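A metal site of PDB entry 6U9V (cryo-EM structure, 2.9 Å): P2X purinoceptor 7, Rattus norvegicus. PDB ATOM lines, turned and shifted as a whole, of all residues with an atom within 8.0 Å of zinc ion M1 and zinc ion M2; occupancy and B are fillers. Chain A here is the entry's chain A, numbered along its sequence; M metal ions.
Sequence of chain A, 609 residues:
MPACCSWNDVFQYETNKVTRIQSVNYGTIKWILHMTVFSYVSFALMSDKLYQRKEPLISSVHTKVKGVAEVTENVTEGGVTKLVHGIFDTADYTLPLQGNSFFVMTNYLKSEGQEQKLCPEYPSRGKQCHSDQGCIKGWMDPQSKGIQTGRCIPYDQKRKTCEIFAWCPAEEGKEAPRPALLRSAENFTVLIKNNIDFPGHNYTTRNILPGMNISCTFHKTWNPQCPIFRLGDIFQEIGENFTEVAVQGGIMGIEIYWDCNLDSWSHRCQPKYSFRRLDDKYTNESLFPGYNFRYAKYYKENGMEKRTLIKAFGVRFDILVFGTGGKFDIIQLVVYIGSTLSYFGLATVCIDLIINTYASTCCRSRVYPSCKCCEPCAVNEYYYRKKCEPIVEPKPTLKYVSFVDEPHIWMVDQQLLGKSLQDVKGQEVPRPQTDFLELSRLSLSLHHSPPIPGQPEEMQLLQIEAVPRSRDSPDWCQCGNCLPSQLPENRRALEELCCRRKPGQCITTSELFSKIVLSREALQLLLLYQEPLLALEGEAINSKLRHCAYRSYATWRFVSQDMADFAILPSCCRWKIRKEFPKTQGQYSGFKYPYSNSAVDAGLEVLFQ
SG of Cys 506 lies close to ND2 of Asn 481, at 3.7 Å. O of Cys 506 lies within hydrogen-bond range of OG1 of Thr 509 (2.6 Å). SG of Cys 479 lies close to N of Asn 481, at 3.7 Å. SG of Cys 498 lies close to N of Gln 478, 3.2 Å away.
N of Gln 478 touches zinc ion M2, at 3.7 Å. The nearest printed residue that does not touch zinc ion M2 is Cys 499 (4.7 Å).
SG of Cys 499 binds zinc ion M1 (2.3 Å). SG of Cys 506 is bound to zinc ion M1, 2.3 Å away. The side-chain sulfur (SG) of Cys 479 binds zinc ion M1, 2.4 Å away. SG of Cys 572 is bound to zinc ion M1, 2.4 Å away.
Within 4 Å of zinc ion M1: Cys 479, Cys 499, Cys 506 and Cys 572.
Zinc ion M2 is bound by the side-chain sulfur of Cys 482 (2.3 Å), the side-chain sulfur of Cys 477 (2.3 Å), the side-chain sulfur of Cys 479 (2.3 Å) and the side-chain sulfur of Cys 498 (2.4 Å).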
ATOM      1  N   GLN A 422     -19.147  -0.901   4.852  1.00  0.00           N
ATOM      2  CA  GLN A 422     -19.735  -1.321   6.118  1.00  0.00           C
ATOM      3  C   GLN A 422     -18.686  -1.418   7.212  1.00  0.00           C
ATOM      4  O   GLN A 422     -18.963  -1.114   8.385  1.00  0.00           O
ATOM      5  CB  GLN A 422     -20.458  -2.666   5.937  1.00  0.00           C
ATOM      6  CG  GLN A 422     -21.668  -2.861   6.837  1.00  0.00           C
ATOM      7  CD  GLN A 422     -21.309  -3.053   8.298  1.00  0.00           C
ATOM      8  OE1 GLN A 422     -20.229  -3.557   8.620  1.00  0.00           O
ATOM      9  NE2 GLN A 422     -22.202  -2.647   9.184  1.00  0.00           N
ATOM     10  N   SER A 473     -27.266 -13.506   0.901  1.00  0.00           N
ATOM     11  CA  SER A 473     -26.891 -12.110   1.038  1.00  0.00           C
ATOM     12  C   SER A 473     -25.459 -11.901   0.533  1.00  0.00           C
ATOM     13  O   SER A 473     -24.727 -12.872   0.298  1.00  0.00           O
ATOM     14  CB  SER A 473     -26.993 -11.677   2.500  1.00  0.00           C
ATOM     15  OG  SER A 473     -28.317 -11.859   2.985  1.00  0.00           O
ATOM     16  N   PRO A 474     -25.031 -10.644   0.340  1.00  0.00           N
ATOM     17  CA  PRO A 474     -23.652 -10.384  -0.069  1.00  0.00           C
ATOM     18  C   PRO A 474     -22.600 -10.726   0.976  1.00  0.00           C
ATOM     19  O   PRO A 474     -21.404 -10.658   0.658  1.00  0.00           O
ATOM     20  CB  PRO A 474     -23.653  -8.880  -0.346  1.00  0.00           C
ATOM     21  CG  PRO A 474     -25.058  -8.525  -0.603  1.00  0.00           C
ATOM     22  CD  PRO A 474     -25.845  -9.413   0.295  1.00  0.00           C
ATOM     23  N   ASP A 475     -22.994 -11.061   2.203  1.00  0.00           N
ATOM     24  CA  ASP A 475     -22.132 -11.480   3.310  1.00  0.00           C
ATOM     25  C   ASP A 475     -21.443 -10.308   4.011  1.00  0.00           C
ATOM     26  O   ASP A 475     -20.710 -10.548   4.981  1.00  0.00           O
ATOM     27  CB  ASP A 475     -21.053 -12.486   2.875  1.00  0.00           C
ATOM     28  N   TRP A 476     -21.653  -9.062   3.568  1.00  0.00           N
ATOM     29  CA  TRP A 476     -21.184  -7.891   4.308  1.00  0.00           C
ATOM     30  C   TRP A 476     -22.290  -7.184   5.085  1.00  0.00           C
ATOM     31  O   TRP A 476     -22.009  -6.204   5.771  1.00  0.00           O
ATOM     32  CB  TRP A 476     -20.492  -6.871   3.369  1.00  0.00           C
ATOM     33  CG  TRP A 476     -21.201  -6.537   2.085  1.00  0.00           C
ATOM     34  CD1 TRP A 476     -20.860  -6.943   0.831  1.00  0.00           C
ATOM     35  CD2 TRP A 476     -22.366  -5.703   1.926  1.00  0.00           C
ATOM     36  NE1 TRP A 476     -21.725  -6.421  -0.097  1.00  0.00           N
ATOM     37  CE2 TRP A 476     -22.665  -5.657   0.555  1.00  0.00           C
ATOM     38  CE3 TRP A 476     -23.177  -4.989   2.814  1.00  0.00           C
ATOM     39  CZ2 TRP A 476     -23.743  -4.938   0.048  1.00  0.00           C
ATOM     40  CZ3 TRP A 476     -24.249  -4.276   2.312  1.00  0.00           C
ATOM     41  CH2 TRP A 476     -24.519  -4.253   0.942  1.00  0.00           C
ATOM     42  N   CYS A 477     -23.533  -7.659   4.986  1.00  0.00           N
ATOM     43  CA  CYS A 477     -24.653  -7.131   5.761  1.00  0.00           C
ATOM     44  C   CYS A 477     -24.993  -8.130   6.858  1.00  0.00           C
ATOM     45  O   CYS A 477     -24.732  -9.328   6.711  1.00  0.00           O
ATOM     46  CB  CYS A 477     -25.887  -6.883   4.883  1.00  0.00           C
ATOM     47  SG  CYS A 477     -27.026  -8.268   4.903  1.00  0.00           S
ATOM     48  N   GLN A 478     -25.582  -7.631   7.944  1.00  0.00           N
ATOM     49  CA  GLN A 478     -25.998  -8.495   9.042  1.00  0.00           C
ATOM     50  C   GLN A 478     -27.482  -8.835   8.938  1.00  0.00           C
ATOM     51  O   GLN A 478     -27.929  -9.866   9.476  1.00  0.00           O
ATOM     52  CB  GLN A 478     -25.699  -7.834  10.382  1.00  0.00           C
ATOM     53  CG  GLN A 478     -24.356  -7.101  10.441  1.00  0.00           C
ATOM     54  CD  GLN A 478     -23.188  -7.977  10.027  1.00  0.00           C
ATOM     55  OE1 GLN A 478     -23.254  -9.203  10.094  1.00  0.00           O
ATOM     56  NE2 GLN A 478     -22.107  -7.336   9.599  1.00  0.00           N
ATOM     57  N   CYS A 479     -28.256  -8.013   8.244  1.00  0.00           N
ATOM     58  CA  CYS A 479     -29.674  -8.253   8.046  1.00  0.00           C
ATOM     59  C   CYS A 479     -29.878  -9.266   6.924  1.00  0.00           C
ATOM     60  O   CYS A 479     -28.932  -9.956   6.540  1.00  0.00           O
ATOM     61  CB  CYS A 479     -30.406  -6.943   7.732  1.00  0.00           C
ATOM     62  SG  CYS A 479     -30.008  -6.223   6.130  1.00  0.00           S
ATOM     63  N   GLY A 480     -31.112  -9.393   6.432  1.00  0.00           N
ATOM     64  CA  GLY A 480     -31.431 -10.292   5.338  1.00  0.00           C
ATOM     65  C   GLY A 480     -31.980  -9.594   4.105  1.00  0.00           C
ATOM     66  O   GLY A 480     -32.044 -10.201   3.030  1.00  0.00           O
ATOM     67  N   ASN A 481     -32.376  -8.330   4.231  1.00  0.00           N
ATOM     68  CA  ASN A 481     -33.040  -7.610   3.147  1.00  0.00           C
ATOM     69  C   ASN A 481     -32.078  -6.911   2.199  1.00  0.00           C
ATOM     70  O   ASN A 481     -32.536  -6.287   1.242  1.00  0.00           O
ATOM     71  CB  ASN A 481     -34.020  -6.598   3.734  1.00  0.00           C
ATOM     72  CG  ASN A 481     -35.198  -7.246   4.427  1.00  0.00           C
ATOM     73  OD1 ASN A 481     -36.275  -7.379   3.846  1.00  0.00           O
ATOM     74  ND2 ASN A 481     -35.002  -7.663   5.670  1.00  0.00           N
ATOM     75  N   CYS A 482     -30.766  -6.973   2.442  1.00  0.00           N
ATOM     76  CA  CYS A 482     -29.824  -6.339   1.536  1.00  0.00           C
ATOM     77  C   CYS A 482     -29.823  -7.042   0.178  1.00  0.00           C
ATOM     78  O   CYS A 482     -30.370  -8.138   0.009  1.00  0.00           O
ATOM     79  CB  CYS A 482     -28.412  -6.349   2.124  1.00  0.00           C
ATOM     80  SG  CYS A 482     -28.086  -5.030   3.326  1.00  0.00           S
ATOM     81  N   LEU A 483     -29.216  -6.386  -0.801  1.00  0.00           N
ATOM     82  CA  LEU A 483     -29.115  -6.887  -2.163  1.00  0.00           C
ATOM     83  C   LEU A 483     -27.817  -6.367  -2.757  1.00  0.00           C
ATOM     84  O   LEU A 483     -27.396  -5.256  -2.417  1.00  0.00           O
ATOM     85  CB  LEU A 483     -30.314  -6.425  -3.009  1.00  0.00           C
ATOM     86  CG  LEU A 483     -30.500  -7.025  -4.406  1.00  0.00           C
ATOM     87  CD1 LEU A 483     -31.058  -8.440  -4.313  1.00  0.00           C
ATOM     88  CD2 LEU A 483     -31.409  -6.146  -5.246  1.00  0.00           C
ATOM     89  N   LEU A 497     -23.284  -1.005   2.079  1.00  0.00           N
ATOM     90  CA  LEU A 497     -23.560  -0.589   3.442  1.00  0.00           C
ATOM     91  C   LEU A 497     -24.802  -1.313   3.937  1.00  0.00           C
ATOM     92  O   LEU A 497     -25.720  -1.585   3.158  1.00  0.00           O
ATOM     93  CB  LEU A 497     -23.749   0.925   3.535  1.00  0.00           C
ATOM     94  CG  LEU A 497     -24.013   1.521   4.923  1.00  0.00           C
ATOM     95  CD1 LEU A 497     -22.824   1.306   5.848  1.00  0.00           C
ATOM     96  CD2 LEU A 497     -24.334   3.001   4.802  1.00  0.00           C
ATOM     97  N   CYS A 498     -24.811  -1.619   5.225  1.00  0.00           N
ATOM     98  CA  CYS A 498     -25.914  -2.323   5.872  1.00  0.00           C
ATOM     99  C   CYS A 498     -26.584  -1.402   6.880  1.00  0.00           C
ATOM    100  O   CYS A 498     -26.129  -0.289   7.153  1.00  0.00           O
ATOM    101  CB  CYS A 498     -25.415  -3.600   6.571  1.00  0.00           C
ATOM    102  SG  CYS A 498     -26.715  -4.781   6.972  1.00  0.00           S
ATOM    103  N   CYS A 499     -27.694  -1.880   7.439  1.00  0.00           N
ATOM    104  CA  CYS A 499     -28.499  -1.097   8.360  1.00  0.00           C
ATOM    105  C   CYS A 499     -28.030  -1.198   9.810  1.00  0.00           C
ATOM    106  O   CYS A 499     -28.565  -0.474  10.659  1.00  0.00           O
ATOM    107  CB  CYS A 499     -29.964  -1.549   8.278  1.00  0.00           C
ATOM    108  SG  CYS A 499     -30.216  -3.303   8.553  1.00  0.00           S
ATOM    109  N   ARG A 500     -27.063  -2.067  10.117  1.00  0.00           N
ATOM    110  CA  ARG A 500     -26.626  -2.228  11.494  1.00  0.00           C
ATOM    111  C   ARG A 500     -25.302  -2.978  11.515  1.00  0.00           C
ATOM    112  O   ARG A 500     -24.881  -3.573  10.522  1.00  0.00           O
ATOM    113  CB  ARG A 500     -27.679  -2.968  12.334  1.00  0.00           C
ATOM    114  CG  ARG A 500     -28.172  -4.289  11.753  1.00  0.00           C
ATOM    115  CD  ARG A 500     -29.396  -4.786  12.503  1.00  0.00           C
ATOM    116  NE  ARG A 500     -29.144  -4.898  13.938  1.00  0.00           N
ATOM    117  CZ  ARG A 500     -30.092  -4.996  14.873  1.00  0.00           C
ATOM    118  NH1 ARG A 500     -31.388  -4.989  14.543  1.00  0.00           N
ATOM    119  NH2 ARG A 500     -29.748  -5.098  16.146  1.00  0.00           N
ATOM    120  N   GLY A 504     -29.635  -8.832  13.670  1.00  0.00           N
ATOM    121  CA  GLY A 504     -30.840  -8.517  14.402  1.00  0.00           C
ATOM    122  C   GLY A 504     -31.973  -8.220  13.444  1.00  0.00           C
ATOM    123  O   GLY A 504     -31.986  -8.680  12.295  1.00  0.00           O
ATOM    124  N   GLN A 505     -32.932  -7.450  13.930  1.00  0.00           N
ATOM    125  CA  GLN A 505     -34.077  -7.049  13.124  1.00  0.00           C
ATOM    126  C   GLN A 505     -33.681  -5.950  12.153  1.00  0.00           C
ATOM    127  O   GLN A 505     -32.955  -5.012  12.521  1.00  0.00           O
ATOM    128  CB  GLN A 505     -35.220  -6.568  14.027  1.00  0.00           C
ATOM    129  CG  GLN A 505     -36.503  -6.213  13.281  1.00  0.00           C
ATOM    130  CD  GLN A 505     -37.634  -5.854  14.218  1.00  0.00           C
ATOM    131  OE1 GLN A 505     -37.537  -6.034  15.432  1.00  0.00           O
ATOM    132  NE2 GLN A 505     -38.727  -5.336  13.659  1.00  0.00           N
ATOM    133  N   CYS A 506     -34.132  -6.064  10.910  1.00  0.00           N
ATOM    134  CA  CYS A 506     -33.846  -5.062   9.905  1.00  0.00           C
ATOM    135  C   CYS A 506     -34.687  -3.814  10.136  1.00  0.00           C
ATOM    136  O   CYS A 506     -35.833  -3.890  10.588  1.00  0.00           O
ATOM    137  CB  CYS A 506     -34.104  -5.615   8.502  1.00  0.00           C
ATOM    138  SG  CYS A 506     -33.408  -4.638   7.156  1.00  0.00           S
ATOM    139  N   ILE A 507     -34.107  -2.653   9.830  1.00  0.00           N
ATOM    140  CA  ILE A 507     -34.797  -1.388  10.066  1.00  0.00           C
ATOM    141  C   ILE A 507     -36.010  -1.245   9.160  1.00  0.00           C
ATOM    142  O   ILE A 507     -36.971  -0.543   9.497  1.00  0.00           O
ATOM    143  CB  ILE A 507     -33.821  -0.209   9.892  1.00  0.00           C
ATOM    144  CG1 ILE A 507     -34.401   1.073  10.492  1.00  0.00           C
ATOM    145  CG2 ILE A 507     -33.495   0.014   8.420  1.00  0.00           C
ATOM    146  CD1 ILE A 507     -33.524   2.284  10.316  1.00  0.00           C
ATOM    147  N   THR A 508     -35.989  -1.895   7.989  1.00  0.00           N
ATOM    148  CA  THR A 508     -37.127  -1.798   7.067  1.00  0.00           C
ATOM    149  C   THR A 508     -38.405  -2.393   7.655  1.00  0.00           C
ATOM    150  O   THR A 508     -39.492  -1.995   7.233  1.00  0.00           O
ATOM    151  CB  THR A 508     -36.789  -2.504   5.750  1.00  0.00           C
ATOM    152  OG1 THR A 508     -37.807  -2.224   4.783  1.00  0.00           O
ATOM    153  CG2 THR A 508     -36.693  -4.020   5.946  1.00  0.00           C
ATOM    154  N   THR A 509     -38.296  -3.322   8.602  1.00  0.00           N
ATOM    155  CA  THR A 509     -39.471  -3.909   9.224  1.00  0.00           C
ATOM    156  C   THR A 509     -40.124  -2.999  10.258  1.00  0.00           C
ATOM    157  O   THR A 509     -41.171  -3.356  10.794  1.00  0.00           O
ATOM    158  CB  THR A 509     -39.102  -5.242   9.885  1.00  0.00           C
ATOM    159  OG1 THR A 509     -38.128  -5.011  10.921  1.00  0.00           O
ATOM    160  CG2 THR A 509     -38.532  -6.211   8.862  1.00  0.00           C
ATOM    161  N   TYR A 553     -35.639   9.592   4.307  1.00  0.00           N
ATOM    162  CA  TYR A 553     -34.860   8.684   5.146  1.00  0.00           C
ATOM    163  C   TYR A 553     -33.629   9.386   5.699  1.00  0.00           C
ATOM    164  O   TYR A 553     -33.246   9.172   6.861  1.00  0.00           O
ATOM    165  CB  TYR A 553     -34.467   7.437   4.359  1.00  0.00           C
ATOM    166  CG  TYR A 553     -33.778   6.379   5.208  1.00  0.00           C
ATOM    167  CD1 TYR A 553     -34.503   5.435   5.898  1.00  0.00           C
ATOM    168  CD2 TYR A 553     -32.394   6.350   5.316  1.00  0.00           C
ATOM    169  CE1 TYR A 553     -33.879   4.477   6.674  1.00  0.00           C
ATOM    170  CE2 TYR A 553     -31.755   5.407   6.080  1.00  0.00           C
ATOM    171  CZ  TYR A 553     -32.505   4.465   6.758  1.00  0.00           C
ATOM    172  OH  TYR A 553     -31.861   3.516   7.527  1.00  0.00           O
ATOM    173  N   PRO A 570     -28.540   2.373   3.395  1.00  0.00           N
ATOM    174  CA  PRO A 570     -28.189   0.952   3.267  1.00  0.00           C
ATOM    175  C   PRO A 570     -28.853   0.311   2.066  1.00  0.00           C
ATOM    176  O   PRO A 570     -29.808   0.833   1.487  1.00  0.00           O
ATOM    177  CB  PRO A 570     -28.710   0.352   4.570  1.00  0.00           C
ATOM    178  CG  PRO A 570     -29.862   1.200   4.932  1.00  0.00           C
ATOM    179  CD  PRO A 570     -29.499   2.592   4.484  1.00  0.00           C
ATOM    180  N   SER A 571     -28.321  -0.849   1.675  1.00  0.00           N
ATOM    181  CA  SER A 571     -28.828  -1.554   0.516  1.00  0.00           C
ATOM    182  C   SER A 571     -30.271  -2.007   0.717  1.00  0.00           C
ATOM    183  O   SER A 571     -31.071  -1.953  -0.217  1.00  0.00           O
ATOM    184  CB  SER A 571     -27.928  -2.746   0.194  1.00  0.00           C
ATOM    185  OG  SER A 571     -28.338  -3.388  -1.005  1.00  0.00           O
ATOM    186  N   CYS A 572     -30.619  -2.450   1.928  1.00  0.00           N
ATOM    187  CA  CYS A 572     -31.953  -2.974   2.186  1.00  0.00           C
ATOM    188  C   CYS A 572     -33.008  -1.884   2.029  1.00  0.00           C
ATOM    189  O   CYS A 572     -34.073  -2.115   1.436  1.00  0.00           O
ATOM    190  CB  CYS A 572     -32.012  -3.584   3.581  1.00  0.00           C
ATOM    191  SG  CYS A 572     -31.114  -2.666   4.857  1.00  0.00           S
ATOM    192  N   CYS A 573     -32.733  -0.682   2.545  1.00  0.00           N
ATOM    193  CA  CYS A 573     -33.686   0.419   2.407  1.00  0.00           C
ATOM    194  C   CYS A 573     -33.642   1.017   1.010  1.00  0.00           C
ATOM    195  O   CYS A 573     -34.679   1.392   0.455  1.00  0.00           O
ATOM    196  CB  CYS A 573     -33.384   1.484   3.457  1.00  0.00           C
ATOM    197  SG  CYS A 573     -33.462   0.889   5.157  1.00  0.00           S
ATOM    198  N   LYS A 576     -35.459  -1.341  -1.281  1.00  0.00           N
ATOM    199  CA  LYS A 576     -36.874  -1.273  -0.946  1.00  0.00           C
ATOM    200  C   LYS A 576     -37.524  -0.057  -1.595  1.00  0.00           C
ATOM    201  O   LYS A 576     -38.584  -0.154  -2.220  1.00  0.00           O
ATOM    202  CB  LYS A 576     -37.064  -1.234   0.572  1.00  0.00           C
ATOM    203  CG  LYS A 576     -37.122  -2.604   1.237  1.00  0.00           C
ATOM    204  CD  LYS A 576     -38.498  -3.227   1.092  1.00  0.00           C
ATOM    205  CE  LYS A 576     -38.553  -4.610   1.717  1.00  0.00           C
ATOM    206  NZ  LYS A 576     -38.249  -4.593   3.169  1.00  0.00           N
HETATM  207 ZN    ZN M   1     -31.164  -4.231   6.641  1.00  0.00          ZN
HETATM  208 ZN    ZN M   2     -27.804  -6.114   5.357  1.00  0.00          ZN
